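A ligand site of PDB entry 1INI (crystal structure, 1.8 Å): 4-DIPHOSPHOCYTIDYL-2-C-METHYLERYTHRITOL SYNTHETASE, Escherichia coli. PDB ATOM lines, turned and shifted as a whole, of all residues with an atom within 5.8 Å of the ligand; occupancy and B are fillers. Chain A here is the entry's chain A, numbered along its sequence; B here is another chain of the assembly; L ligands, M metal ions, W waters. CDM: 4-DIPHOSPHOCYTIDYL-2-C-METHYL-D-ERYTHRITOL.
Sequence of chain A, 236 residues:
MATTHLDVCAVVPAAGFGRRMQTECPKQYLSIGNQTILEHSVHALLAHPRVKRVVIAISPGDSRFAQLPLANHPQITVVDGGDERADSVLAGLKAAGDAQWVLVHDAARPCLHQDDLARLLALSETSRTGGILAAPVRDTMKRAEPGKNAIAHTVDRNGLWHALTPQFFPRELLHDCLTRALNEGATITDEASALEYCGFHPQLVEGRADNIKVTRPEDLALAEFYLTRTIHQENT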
ATOM      1  N   VAL A  12     -23.021 -13.501  15.109  1.00  0.00           N
ATOM      2  CA  VAL A  12     -22.808 -14.240  16.342  1.00  0.00           C
ATOM      3  C   VAL A  12     -21.556 -15.126  16.249  1.00  0.00           C
ATOM      4  O   VAL A  12     -21.550 -16.152  15.565  1.00  0.00           O
ATOM      5  CB  VAL A  12     -24.034 -15.153  16.687  1.00  0.00           C
ATOM      6  CG1 VAL A  12     -23.700 -16.137  17.808  1.00  0.00           C
ATOM      7  CG2 VAL A  12     -25.210 -14.277  17.062  1.00  0.00           C
ATOM      8  N   PRO A  13     -20.464 -14.713  16.925  1.00  0.00           N
ATOM      9  CA  PRO A  13     -19.248 -15.514  16.879  1.00  0.00           C
ATOM     10  C   PRO A  13     -19.472 -16.751  17.759  1.00  0.00           C
ATOM     11  O   PRO A  13     -19.723 -16.628  18.960  1.00  0.00           O
ATOM     12  CB  PRO A  13     -18.178 -14.555  17.437  1.00  0.00           C
ATOM     13  CG  PRO A  13     -18.941 -13.592  18.319  1.00  0.00           C
ATOM     14  CD  PRO A  13     -20.226 -13.382  17.505  1.00  0.00           C
ATOM     15  N   ALA A  14     -19.426 -17.922  17.139  1.00  0.00           N
ATOM     16  CA  ALA A  14     -19.665 -19.184  17.837  1.00  0.00           C
ATOM     17  C   ALA A  14     -18.702 -20.258  17.349  1.00  0.00           C
ATOM     18  O   ALA A  14     -19.069 -21.441  17.272  1.00  0.00           O
ATOM     19  CB  ALA A  14     -21.091 -19.637  17.604  1.00  0.00           C
ATOM     20  N   ALA A  15     -17.490 -19.856  17.010  1.00  0.00           N
ATOM     21  CA  ALA A  15     -16.502 -20.787  16.486  1.00  0.00           C
ATOM     22  C   ALA A  15     -15.483 -21.206  17.543  1.00  0.00           C
ATOM     23  O   ALA A  15     -14.518 -21.894  17.222  1.00  0.00           O
ATOM     24  CB  ALA A  15     -15.787 -20.157  15.291  1.00  0.00           C
ATOM     25  N   GLY A  16     -15.699 -20.776  18.780  1.00  0.00           N
ATOM     26  CA  GLY A  16     -14.802 -21.134  19.850  1.00  0.00           C
ATOM     27  C   GLY A  16     -14.893 -22.603  20.213  1.00  0.00           C
ATOM     28  O   GLY A  16     -15.975 -23.194  20.205  1.00  0.00           O
ATOM     29  N   PHE A  17     -13.740 -23.193  20.523  1.00  0.00           N
ATOM     30  CA  PHE A  17     -13.667 -24.608  20.903  1.00  0.00           C
ATOM     31  C   PHE A  17     -13.904 -24.678  22.410  1.00  0.00           C
ATOM     32  O   PHE A  17     -14.172 -25.754  22.970  1.00  0.00           O
ATOM     33  CB  PHE A  17     -12.281 -25.158  20.560  1.00  0.00           C
ATOM     34  CG  PHE A  17     -11.926 -25.035  19.109  1.00  0.00           C
ATOM     35  CD1 PHE A  17     -10.601 -25.194  18.687  1.00  0.00           C
ATOM     36  CD2 PHE A  17     -12.900 -24.736  18.160  1.00  0.00           C
ATOM     37  CE1 PHE A  17     -10.259 -25.064  17.352  1.00  0.00           C
ATOM     38  CE2 PHE A  17     -12.568 -24.598  16.818  1.00  0.00           C
ATOM     39  CZ  PHE A  17     -11.240 -24.759  16.406  1.00  0.00           C
ATOM     40  N   ARG A  20     -11.887 -24.473  28.145  1.00  0.00           N
ATOM     41  CA  ARG A  20     -11.916 -23.884  29.478  1.00  0.00           C
ATOM     42  C   ARG A  20     -13.225 -24.435  30.011  1.00  0.00           C
ATOM     43  O   ARG A  20     -13.706 -24.066  31.096  1.00  0.00           O
ATOM     44  CB  ARG A  20     -11.949 -22.356  29.400  1.00  0.00           C
ATOM     45  CG  ARG A  20     -10.569 -21.705  29.285  1.00  0.00           C
ATOM     46  CD  ARG A  20     -10.654 -20.191  29.269  1.00  0.00           C
ATOM     47  NE  ARG A  20     -11.355 -19.707  28.081  1.00  0.00           N
ATOM     48  CZ  ARG A  20     -11.645 -18.432  27.847  1.00  0.00           C
ATOM     49  NH1 ARG A  20     -11.298 -17.491  28.714  1.00  0.00           N
ATOM     50  NH2 ARG A  20     -12.272 -18.096  26.730  1.00  0.00           N
ATOM     51  N   LYS A  27     -19.306 -25.184  24.831  1.00  0.00           N
ATOM     52  CA  LYS A  27     -20.192 -24.512  25.759  1.00  0.00           C
ATOM     53  C   LYS A  27     -21.483 -24.021  25.090  1.00  0.00           C
ATOM     54  O   LYS A  27     -22.564 -24.106  25.677  1.00  0.00           O
ATOM     55  CB  LYS A  27     -19.446 -23.350  26.407  1.00  0.00           C
ATOM     56  CG  LYS A  27     -18.721 -22.459  25.402  1.00  0.00           C
ATOM     57  CD  LYS A  27     -17.702 -21.532  26.063  1.00  0.00           C
ATOM     58  CE  LYS A  27     -16.909 -20.744  25.018  1.00  0.00           C
ATOM     59  NZ  LYS A  27     -15.905 -19.856  25.648  1.00  0.00           N
ATOM     60  N   GLN A  28     -21.372 -23.493  23.875  1.00  0.00           N
ATOM     61  CA  GLN A  28     -22.563 -22.996  23.189  1.00  0.00           C
ATOM     62  C   GLN A  28     -23.569 -24.095  22.849  1.00  0.00           C
ATOM     63  O   GLN A  28     -24.752 -23.829  22.609  1.00  0.00           O
ATOM     64  CB  GLN A  28     -22.198 -22.224  21.903  1.00  0.00           C
ATOM     65  CG  GLN A  28     -21.443 -23.036  20.847  1.00  0.00           C
ATOM     66  CD  GLN A  28     -19.927 -22.996  21.046  1.00  0.00           C
ATOM     67  OE1 GLN A  28     -19.428 -23.162  22.160  1.00  0.00           O
ATOM     68  NE2 GLN A  28     -19.203 -22.783  19.958  1.00  0.00           N
ATOM     69  N   ALA A  57     -21.081 -17.572  12.933  1.00  0.00           N
ATOM     70  CA  ALA A  57     -19.761 -18.082  12.534  1.00  0.00           C
ATOM     71  C   ALA A  57     -19.463 -19.299  13.413  1.00  0.00           C
ATOM     72  O   ALA A  57     -19.522 -19.212  14.641  1.00  0.00           O
ATOM     73  CB  ALA A  57     -18.697 -17.014  12.739  1.00  0.00           C
ATOM     74  N   GLY A  81     -15.852 -19.568  11.116  1.00  0.00           N
ATOM     75  CA  GLY A  81     -15.152 -18.579  11.923  1.00  0.00           C
ATOM     76  C   GLY A  81     -13.646 -18.682  11.729  1.00  0.00           C
ATOM     77  O   GLY A  81     -13.195 -19.408  10.850  1.00  0.00           O
ATOM     78  N   GLY A  82     -12.879 -17.958  12.553  1.00  0.00           N
ATOM     79  CA  GLY A  82     -11.418 -17.972  12.442  1.00  0.00           C
ATOM     80  C   GLY A  82     -10.674 -18.389  13.707  1.00  0.00           C
ATOM     81  O   GLY A  82     -11.282 -18.899  14.637  1.00  0.00           O
ATOM     82  N   ASP A  83      -9.368 -18.151  13.755  1.00  0.00           N
ATOM     83  CA  ASP A  83      -8.568 -18.557  14.913  1.00  0.00           C
ATOM     84  C   ASP A  83      -8.971 -17.900  16.219  1.00  0.00           C
ATOM     85  O   ASP A  83      -9.036 -18.566  17.247  1.00  0.00           O
ATOM     86  CB  ASP A  83      -7.085 -18.304  14.663  1.00  0.00           C
ATOM     87  CG  ASP A  83      -6.584 -18.966  13.392  1.00  0.00           C
ATOM     88  OD1 ASP A  83      -7.128 -20.030  13.034  1.00  0.00           O
ATOM     89  OD2 ASP A  83      -5.645 -18.420  12.758  1.00  0.00           O
ATOM     90  N   GLU A  84      -9.201 -16.598  16.181  1.00  0.00           N
ATOM     91  CA  GLU A  84      -9.598 -15.862  17.376  1.00  0.00           C
ATOM     92  C   GLU A  84     -10.999 -15.285  17.175  1.00  0.00           C
ATOM     93  O   GLU A  84     -11.544 -15.285  16.049  1.00  0.00           O
ATOM     94  CB  GLU A  84      -8.600 -14.743  17.658  1.00  0.00           C
ATOM     95  CG  GLU A  84      -7.200 -15.226  18.012  1.00  0.00           C
ATOM     96  CD  GLU A  84      -7.189 -16.054  19.271  1.00  0.00           C
ATOM     97  OE1 GLU A  84      -7.636 -15.550  20.326  1.00  0.00           O
ATOM     98  OE2 GLU A  84      -6.721 -17.216  19.231  1.00  0.00           O
ATOM     99  N   ARG A  85     -11.581 -14.777  18.253  1.00  0.00           N
ATOM    100  CA  ARG A  85     -12.932 -14.202  18.173  1.00  0.00           C
ATOM    101  C   ARG A  85     -13.009 -13.105  17.104  1.00  0.00           C
ATOM    102  O   ARG A  85     -13.916 -13.116  16.274  1.00  0.00           O
ATOM    103  CB  ARG A  85     -13.343 -13.628  19.527  1.00  0.00           C
ATOM    104  CG  ARG A  85     -14.764 -13.042  19.574  1.00  0.00           C
ATOM    105  CD  ARG A  85     -15.110 -12.541  20.969  1.00  0.00           C
ATOM    106  NE  ARG A  85     -16.458 -11.971  21.028  1.00  0.00           N
ATOM    107  CZ  ARG A  85     -16.784 -10.779  20.548  1.00  0.00           C
ATOM    108  NH1 ARG A  85     -15.845 -10.026  19.994  1.00  0.00           N
ATOM    109  NH2 ARG A  85     -18.037 -10.340  20.618  1.00  0.00           N
ATOM    110  N   SER A  88     -13.454 -14.540  13.698  1.00  0.00           N
ATOM    111  CA  SER A  88     -14.787 -15.100  13.447  1.00  0.00           C
ATOM    112  C   SER A  88     -15.777 -13.955  13.206  1.00  0.00           C
ATOM    113  O   SER A  88     -16.642 -14.038  12.339  1.00  0.00           O
ATOM    114  CB  SER A  88     -15.228 -15.956  14.635  1.00  0.00           C
ATOM    115  OG  SER A  88     -14.290 -16.991  14.900  1.00  0.00           O
ATOM    116  N   VAL A  89     -15.640 -12.887  13.990  1.00  0.00           N
ATOM    117  CA  VAL A  89     -16.527 -11.732  13.850  1.00  0.00           C
ATOM    118  C   VAL A  89     -16.361 -11.070  12.488  1.00  0.00           C
ATOM    119  O   VAL A  89     -17.345 -10.647  11.851  1.00  0.00           O
ATOM    120  CB  VAL A  89     -16.259 -10.708  14.998  1.00  0.00           C
ATOM    121  CG1 VAL A  89     -16.999  -9.392  14.722  1.00  0.00           C
ATOM    122  CG2 VAL A  89     -16.718 -11.312  16.344  1.00  0.00           C
ATOM    123  N   ASP A 106     -22.005 -12.364  21.525  1.00  0.00           N
ATOM    124  CA  ASP A 106     -21.391 -13.663  21.843  1.00  0.00           C
ATOM    125  C   ASP A 106     -22.413 -14.786  21.897  1.00  0.00           C
ATOM    126  O   ASP A 106     -23.491 -14.660  22.497  1.00  0.00           O
ATOM    127  CB  ASP A 106     -20.708 -13.656  23.230  1.00  0.00           C
ATOM    128  CG  ASP A 106     -19.507 -12.733  23.307  1.00  0.00           C
ATOM    129  OD1 ASP A 106     -18.825 -12.529  22.288  1.00  0.00           O
ATOM    130  OD2 ASP A 106     -19.249 -12.212  24.418  1.00  0.00           O
ATOM    131  N   ALA A 107     -22.103 -15.918  21.262  1.00  0.00           N
ATOM    132  CA  ALA A 107     -23.035 -17.050  21.311  1.00  0.00           C
ATOM    133  C   ALA A 107     -23.207 -17.507  22.777  1.00  0.00           C
ATOM    134  O   ALA A 107     -24.259 -18.000  23.181  1.00  0.00           O
ATOM    135  CB  ALA A 107     -22.506 -18.188  20.501  1.00  0.00           C
ATOM    136  N   ALA A 108     -22.152 -17.293  23.562  1.00  0.00           N
ATOM    137  CA  ALA A 108     -22.091 -17.704  24.972  1.00  0.00           C
ATOM    138  C   ALA A 108     -22.798 -16.830  26.005  1.00  0.00           C
ATOM    139  O   ALA A 108     -22.644 -17.041  27.219  1.00  0.00           O
ATOM    140  CB  ALA A 108     -20.642 -17.865  25.358  1.00  0.00           C
ATOM    141  N   ARG A 109     -23.555 -15.840  25.554  1.00  0.00           N
ATOM    142  CA  ARG A 109     -24.297 -14.982  26.469  1.00  0.00           C
ATOM    143  C   ARG A 109     -25.779 -15.160  26.185  1.00  0.00           C
ATOM    144  O   ARG A 109     -26.394 -14.330  25.526  1.00  0.00           O
ATOM    145  CB  ARG A 109     -23.885 -13.517  26.291  1.00  0.00           C
ATOM    146  CG  ARG A 109     -22.505 -13.164  26.822  1.00  0.00           C
ATOM    147  CD  ARG A 109     -22.244 -11.681  26.609  1.00  0.00           C
ATOM    148  NE  ARG A 109     -20.866 -11.282  26.941  1.00  0.00           N
ATOM    149  CZ  ARG A 109     -20.409 -11.104  28.179  1.00  0.00           C
ATOM    150  NH1 ARG A 109     -21.210 -11.272  29.239  1.00  0.00           N
ATOM    151  NH2 ARG A 109     -19.147 -10.731  28.359  1.00  0.00           N
ATOM    152  N   HIS A 162     -17.563  -3.237  32.812  1.00  0.00           N
ATOM    153  CA  HIS A 162     -17.482  -4.583  32.286  1.00  0.00           C
ATOM    154  C   HIS A 162     -18.093  -4.461  30.887  1.00  0.00           C
ATOM    155  O   HIS A 162     -19.246  -4.072  30.758  1.00  0.00           O
ATOM    156  CB  HIS A 162     -18.403  -5.534  33.047  1.00  0.00           C
ATOM    157  CG  HIS A 162     -17.855  -6.027  34.349  1.00  0.00           C
ATOM    158  ND1 HIS A 162     -17.027  -7.135  34.432  1.00  0.00           N
ATOM    159  CD2 HIS A 162     -18.065  -5.622  35.623  1.00  0.00           C
ATOM    160  CE1 HIS A 162     -16.766  -7.383  35.707  1.00  0.00           C
ATOM    161  NE2 HIS A 162     -17.385  -6.487  36.447  1.00  0.00           N
ATOM    162  N   ALA A 163     -17.345  -4.780  29.831  1.00  0.00           N
ATOM    163  CA  ALA A 163     -17.943  -4.709  28.507  1.00  0.00           C
ATOM    164  C   ALA A 163     -18.737  -6.011  28.305  1.00  0.00           C
ATOM    165  O   ALA A 163     -18.239  -7.112  28.608  1.00  0.00           O
ATOM    166  CB  ALA A 163     -16.859  -4.562  27.450  1.00  0.00           C
ATOM    167  N   LEU A 164     -19.966  -5.891  27.827  1.00  0.00           N
ATOM    168  CA  LEU A 164     -20.790  -7.057  27.567  1.00  0.00           C
ATOM    169  C   LEU A 164     -21.132  -7.017  26.072  1.00  0.00           C
ATOM    170  O   LEU A 164     -20.536  -6.271  25.318  1.00  0.00           O
ATOM    171  CB  LEU A 164     -22.077  -6.950  28.390  1.00  0.00           C
ATOM    172  CG  LEU A 164     -21.906  -6.709  29.892  1.00  0.00           C
ATOM    173  CD1 LEU A 164     -23.247  -6.417  30.532  1.00  0.00           C
ATOM    174  CD2 LEU A 164     -21.261  -7.935  30.554  1.00  0.00           C
ATOM    175  N   THR A 165     -22.082  -7.837  25.656  1.00  0.00           N
ATOM    176  CA  THR A 165     -22.545  -7.815  24.261  1.00  0.00           C
ATOM    177  C   THR A 165     -24.046  -8.012  24.384  1.00  0.00           C
ATOM    178  O   THR A 165     -24.540  -8.519  25.387  1.00  0.00           O
ATOM    179  CB  THR A 165     -21.908  -8.926  23.336  1.00  0.00           C
ATOM    180  OG1 THR A 165     -22.447 -10.199  23.675  1.00  0.00           O
ATOM    181  CG2 THR A 165     -20.377  -8.950  23.434  1.00  0.00           C
ATOM    182  N   GLN A 167     -22.862  -5.578  20.968  1.00  0.00           N
ATOM    183  CA  GLN A 167     -22.090  -4.381  20.667  1.00  0.00           C
ATOM    184  C   GLN A 167     -22.677  -3.986  19.303  1.00  0.00           C
ATOM    185  O   GLN A 167     -22.715  -4.795  18.382  1.00  0.00           O
ATOM    186  CB  GLN A 167     -20.603  -4.723  20.613  1.00  0.00           C
ATOM    187  CG  GLN A 167     -20.161  -5.275  21.983  1.00  0.00           C
ATOM    188  CD  GLN A 167     -18.674  -5.029  22.306  1.00  0.00           C
ATOM    189  OE1 GLN A 167     -17.894  -4.592  21.451  1.00  0.00           O
ATOM    190  NE2 GLN A 167     -18.293  -5.309  23.561  1.00  0.00           N
ATOM    191  N   THR A 189     -10.179  -7.577  21.766  1.00  0.00           N
ATOM    192  CA  THR A 189     -10.984  -8.518  22.526  1.00  0.00           C
ATOM    193  C   THR A 189     -12.491  -8.321  22.385  1.00  0.00           C
ATOM    194  O   THR A 189     -13.293  -9.119  22.890  1.00  0.00           O
ATOM    195  CB  THR A 189     -10.616  -8.496  24.019  1.00  0.00           C
ATOM    196  OG1 THR A 189     -10.808  -7.181  24.542  1.00  0.00           O
ATOM    197  CG2 THR A 189      -9.155  -8.905  24.195  1.00  0.00           C
ATOM    198  N   ASP A 190     -12.877  -7.237  21.742  1.00  0.00           N
ATOM    199  CA  ASP A 190     -14.280  -7.003  21.456  1.00  0.00           C
ATOM    200  C   ASP A 190     -14.370  -6.031  20.279  1.00  0.00           C
ATOM    201  O   ASP A 190     -13.344  -5.630  19.733  1.00  0.00           O
ATOM    202  CB  ASP A 190     -15.073  -6.545  22.700  1.00  0.00           C
ATOM    203  CG  ASP A 190     -14.762  -5.153  23.150  1.00  0.00           C
ATOM    204  OD1 ASP A 190     -13.827  -4.503  22.638  1.00  0.00           O
ATOM    205  OD2 ASP A 190     -15.496  -4.680  24.067  1.00  0.00           O
ATOM    206  N   GLU A 191     -15.579  -5.710  19.839  1.00  0.00           N
ATOM    207  CA  GLU A 191     -15.743  -4.818  18.682  1.00  0.00           C
ATOM    208  C   GLU A 191     -15.472  -3.370  19.025  1.00  0.00           C
ATOM    209  O   GLU A 191     -14.994  -2.597  18.181  1.00  0.00           O
ATOM    210  CB  GLU A 191     -17.151  -4.944  18.104  1.00  0.00           C
ATOM    211  CG  GLU A 191     -17.408  -6.273  17.423  1.00  0.00           C
ATOM    212  CD  GLU A 191     -17.209  -7.464  18.377  1.00  0.00           C
ATOM    213  OE1 GLU A 191     -17.894  -7.536  19.424  1.00  0.00           O
ATOM    214  OE2 GLU A 191     -16.381  -8.333  18.066  1.00  0.00           O
ATOM    215  N   LYS A 213     -21.417 -14.483  30.506  1.00  0.00           N
ATOM    216  CA  LYS A 213     -20.798 -15.282  29.452  1.00  0.00           C
ATOM    217  C   LYS A 213     -20.461 -16.668  30.023  1.00  0.00           C
ATOM    218  O   LYS A 213     -19.806 -16.771  31.060  1.00  0.00           O
ATOM    219  CB  LYS A 213     -19.515 -14.611  28.966  1.00  0.00           C
ATOM    220  CG  LYS A 213     -18.832 -15.329  27.811  1.00  0.00           C
ATOM    221  CD  LYS A 213     -17.590 -14.589  27.307  1.00  0.00           C
ATOM    222  CE  LYS A 213     -16.390 -14.793  28.232  1.00  0.00           C
ATOM    223  NZ  LYS A 213     -16.055 -13.557  28.989  1.00  0.00           N
ATOM    224  N   VAL A 214     -20.939 -17.720  29.357  1.00  0.00           N
ATOM    225  CA  VAL A 214     -20.685 -19.087  29.800  1.00  0.00           C
ATOM    226  C   VAL A 214     -19.381 -19.585  29.193  1.00  0.00           C
ATOM    227  O   VAL A 214     -19.323 -19.874  27.995  1.00  0.00           O
ATOM    228  CB  VAL A 214     -21.831 -20.029  29.373  1.00  0.00           C
ATOM    229  CG1 VAL A 214     -21.522 -21.467  29.829  1.00  0.00           C
ATOM    230  CG2 VAL A 214     -23.143 -19.551  29.981  1.00  0.00           C
ATOM    231  N   THR A 215     -18.343 -19.707  30.008  1.00  0.00           N
ATOM    232  CA  THR A 215     -17.050 -20.171  29.518  1.00  0.00           C
ATOM    233  C   THR A 215     -16.539 -21.359  30.315  1.00  0.00           C
ATOM    234  O   THR A 215     -15.919 -22.273  29.768  1.00  0.00           O
ATOM    235  CB  THR A 215     -15.991 -19.058  29.612  1.00  0.00           C
ATOM    236  OG1 THR A 215     -16.571 -17.798  29.231  1.00  0.00           O
ATOM    237  CG2 THR A 215     -14.833 -19.363  28.675  1.00  0.00           C
ATOM    238  N   ARG B 138     -12.465 -11.496  33.619  1.00  0.00           N
ATOM    239  CA  ARG B 138     -12.826 -12.227  32.403  1.00  0.00           C
ATOM    240  C   ARG B 138     -13.313 -11.346  31.244  1.00  0.00           C
ATOM    241  O   ARG B 138     -12.902 -11.547  30.111  1.00  0.00           O
ATOM    242  CB  ARG B 138     -13.914 -13.258  32.712  1.00  0.00           C
ATOM    243  CG  ARG B 138     -13.535 -14.323  33.728  1.00  0.00           C
ATOM    244  CD  ARG B 138     -14.710 -15.285  33.907  1.00  0.00           C
ATOM    245  NE  ARG B 138     -14.394 -16.391  34.814  1.00  0.00           N
ATOM    246  CZ  ARG B 138     -15.076 -17.526  34.859  1.00  0.00           C
ATOM    247  NH1 ARG B 138     -16.109 -17.711  34.047  1.00  0.00           N
ATOM    248  NH2 ARG B 138     -14.705 -18.483  35.708  1.00  0.00           N
ATOM    249  N   ASP B 139     -14.194 -10.384  31.523  1.00  0.00           N
ATOM    250  CA  ASP B 139     -14.690  -9.539  30.460  1.00  0.00           C
ATOM    251  C   ASP B 139     -13.682  -8.484  30.046  1.00  0.00           C
ATOM    252  O   ASP B 139     -12.735  -8.183  30.777  1.00  0.00           O
ATOM    253  CB  ASP B 139     -15.956  -8.793  30.877  1.00  0.00           C
ATOM    254  CG  ASP B 139     -17.112  -9.715  31.151  1.00  0.00           C
ATOM    255  OD1 ASP B 139     -17.234 -10.733  30.433  1.00  0.00           O
ATOM    256  OD2 ASP B 139     -17.898  -9.386  32.060  1.00  0.00           O
ATOM    257  N   THR B 140     -13.904  -7.913  28.872  1.00  0.00           N
ATOM    258  CA  THR B 140     -13.047  -6.831  28.403  1.00  0.00           C
ATOM    259  C   THR B 140     -13.463  -5.700  29.340  1.00  0.00           C
ATOM    260  O   THR B 140     -14.652  -5.550  29.630  1.00  0.00           O
ATOM    261  CB  THR B 140     -13.369  -6.454  26.941  1.00  0.00           C
ATOM    262  OG1 THR B 140     -12.907  -7.503  26.082  1.00  0.00           O
ATOM    263  CG2 THR B 140     -12.690  -5.159  26.526  1.00  0.00           C
ATOM    264  N   ARG B 157      -7.369  -6.565  30.506  1.00  0.00           N
ATOM    265  CA  ARG B 157      -7.865  -7.534  31.485  1.00  0.00           C
ATOM    266  C   ARG B 157      -6.793  -8.520  31.940  1.00  0.00           C
ATOM    267  O   ARG B 157      -6.964  -9.230  32.940  1.00  0.00           O
ATOM    268  CB  ARG B 157      -9.058  -8.331  30.921  1.00  0.00           C
ATOM    269  CG  ARG B 157      -8.732  -9.165  29.698  1.00  0.00           C
ATOM    270  CD  ARG B 157      -9.943  -9.907  29.192  1.00  0.00           C
ATOM    271  NE  ARG B 157      -9.701 -10.535  27.899  1.00  0.00           N
ATOM    272  CZ  ARG B 157     -10.655 -11.015  27.105  1.00  0.00           C
ATOM    273  NH1 ARG B 157     -11.925 -10.928  27.485  1.00  0.00           N
ATOM    274  NH2 ARG B 157     -10.340 -11.575  25.943  1.00  0.00           N
HETATM  275  N1  CDM L   1     -15.323 -17.227  19.461  1.00  0.00           N
HETATM  276  C2  CDM L   1     -15.297 -17.488  18.052  1.00  0.00           C
HETATM  277  N3  CDM L   1     -14.136 -17.820  17.425  1.00  0.00           N
HETATM  278  C4  CDM L   1     -12.907 -17.913  18.178  1.00  0.00           C
HETATM  279  C5  CDM L   1     -12.861 -17.659  19.580  1.00  0.00           C
HETATM  280  C6  CDM L   1     -14.077 -17.324  20.164  1.00  0.00           C
HETATM  281  O2  CDM L   1     -16.301 -17.440  17.311  1.00  0.00           O
HETATM  282  N4  CDM L   1     -11.789 -18.244  17.503  1.00  0.00           N
HETATM  283  C1' CDM L   1     -16.580 -16.865  20.185  1.00  0.00           C
HETATM  284  C2' CDM L   1     -16.949 -17.928  21.209  1.00  0.00           C
HETATM  285  O2' CDM L   1     -17.486 -19.028  20.518  1.00  0.00           O
HETATM  286  C3' CDM L   1     -17.861 -17.200  22.176  1.00  0.00           C
HETATM  287  C4' CDM L   1     -17.452 -15.720  21.990  1.00  0.00           C
HETATM  288  O4' CDM L   1     -16.455 -15.687  20.943  1.00  0.00           O
HETATM  289  O3' CDM L   1     -19.254 -17.245  21.808  1.00  0.00           O
HETATM  290  C5' CDM L   1     -16.862 -15.293  23.325  1.00  0.00           C
HETATM  291  O5' CDM L   1     -15.652 -15.955  23.505  1.00  0.00           O
HETATM  292  PA  CDM L   1     -14.955 -16.261  24.956  1.00  0.00           P
HETATM  293  O1A CDM L   1     -16.102 -16.954  25.796  1.00  0.00           O
HETATM  294  O2A CDM L   1     -13.616 -17.263  24.608  1.00  0.00           O
HETATM  295  O3A CDM L   1     -14.589 -14.914  25.454  1.00  0.00           O
HETATM  296  PB  CDM L   1     -13.612 -13.791  25.289  1.00  0.00           P
HETATM  297  O1B CDM L   1     -13.304 -13.599  23.843  1.00  0.00           O
HETATM  298  O2B CDM L   1     -12.355 -14.184  26.102  1.00  0.00           O
HETATM  299  O3B CDM L   1     -13.945 -12.397  25.715  1.00  0.00           O
HETATM  300  C1M CDM L   1     -15.109 -11.874  25.109  1.00  0.00           C
HETATM  301  C2M CDM L   1     -15.314 -10.518  25.761  1.00  0.00           C
HETATM  302  O2M CDM L   1     -14.122  -9.681  25.344  1.00  0.00           O
HETATM  303  C3M CDM L   1     -16.637  -9.781  25.332  1.00  0.00           C
HETATM  304  C4M CDM L   1     -16.600  -8.429  25.996  1.00  0.00           C
HETATM  305  C5M CDM L   1     -16.765  -9.687  23.790  1.00  0.00           C
HETATM  306  O3M CDM L   1     -17.862 -10.477  25.889  1.00  0.00           O
HETATM  307  O4M CDM L   1     -16.564  -8.585  27.546  1.00  0.00           O
HETATM  308 MG    MG M   1     -11.224 -17.371  23.438  1.00  0.00          MG
HETATM  309  O   HOH W   1      -9.531 -18.678  19.981  1.00  0.00           O
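O2A of the ligand lies within salt-bridge range of NH2 of Arg 20 (2.6 Å).
O3' of the ligand is in hydrogen-bond range of N of Ala 107, at 3.2 Å.
OG1 of Thr 140 of chain B lies within hydrogen-bond range of O2M of the ligand (2.6 Å).
O of Glu 84 sits close to N4 of the ligand (3.3 Å).
A nitrogen (N3) of the ligand sits at hydrogen-bond distance from the side-chain hydroxyl (OG) of Ser 88, 2.7 Å away.
The backbone carbonyl oxygen of Pro 13 is in hydrogen-bond range of an oxygen (O3') of the ligand.
N of Ala 108 is in hydrogen-bond range of O3' of the ligand (3.4 Å).
An oxygen (O2) of the ligand lies within hydrogen-bond range of the backbone NH (N) of Ala 14.
OD2 of Asp 106 is in hydrogen-bond range of O3M of the ligand (2.7 Å).
The backbone carbonyl oxygen (O) of Thr 189 lies within hydrogen-bond range of an oxygen (O2M) of the ligand.
An oxygen (O2) of the ligand sits at hydrogen-bond distance from the backbone NH of Ala 15 (2.7 Å).
N of Thr 140 of chain B lies within hydrogen-bond range of O4M of the ligand (3.0 Å).
The backbone NH (N) of Gly 16 lies within hydrogen-bond range of an oxygen (O2') of the ligand.
A nitrogen (N4) of the ligand is in hydrogen-bond range of the backbone carbonyl oxygen of Gly 82 (3.0 Å).
O of Ala 163 sits at hydrogen-bond distance from O4M of the ligand, at 2.5 Å.
An oxygen (O2B) of the ligand lies within salt-bridge range of the guanidinium group of Arg 157 of chain B (3.3 Å).
An oxygen (O3M) of the ligand lies within hydrogen-bond range of the guanidinium group (NH2) of Arg 109 (2.8 Å).
The side-chain amino group of Lys 27 lies within salt-bridge range of an oxygen (O1A) of the ligand.
A nitrogen (N4) of the ligand lies within hydrogen-bond range of the backbone carbonyl oxygen (O) of Asp 83 (2.8 Å).
Arg 85 touches the ligand (N to C4, 3.4 Å).
Thr 165 touches the ligand.
CB of Asp 190 touches C5M of the ligand (3.7 Å).
Lys 213 touches the ligand (CD to O1A, 3.2 Å).
OG1 of Thr 215 touches O1A of the ligand, at 3.6 Å.
Asp 139 of chain B touches the ligand.
Hydrophobic or aromatic side chains within 4 Å of the ligand: Pro 13, Ala 15, Ala 107 and Ala 108.
Within 4 Å of the ligand: Pro 13, Ala 14, Ala 15, Gly 16, Arg 20, Lys 27, Gly 82, Asp 83, Glu 84, Arg 85, Ser 88, Asp 106, Ala 107, Ala 108, Arg 109, Ala 163, Thr 165, Thr 189, Asp 190, Lys 213, Thr 215, Asp 139 of chain B, Thr 140 of chain B and Arg 157 of chain B.
The nearest printed residue that does not touch the ligand is Gln 28 (4.2 Å).
N of Ala 15 lies within hydrogen-bond range of O of Ala 57 (3.2 Å).
The backbone NH (N) of Asp 106 is in hydrogen-bond range of the side-chain hydroxyl (OG1) of Thr 165.
A ring nitrogen (ND1) of His 162 is in hydrogen-bond range of the side-chain carboxylate of Asp 139 of chain B (3.4 Å).
OD2 of Asp 190 sits at hydrogen-bond distance from NE2 of Gln 167.
N of Ala 14 lies within hydrogen-bond range of O of Ala 57 (2.8 Å).
The side-chain amide nitrogen (NE2) of Gln 28 lies within hydrogen-bond range of the backbone carbonyl oxygen (O) of Gly 16 (3.3 Å).
OD1 of Asp 106 lies within salt-bridge range of NE of Arg 85 (2.7 Å).
The backbone NH of Gly 82 sits at hydrogen-bond distance from the side-chain hydroxyl of Ser 88 (2.9 Å).
Water W1 lies within hydrogen-bond range of the backbone carbonyl oxygen (O) of Asp 83 (2.8 Å), the side-chain carboxylate (OE2) of Glu 84 (3.3 Å) and a nitrogen (N4) of the ligand (3.4 Å).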
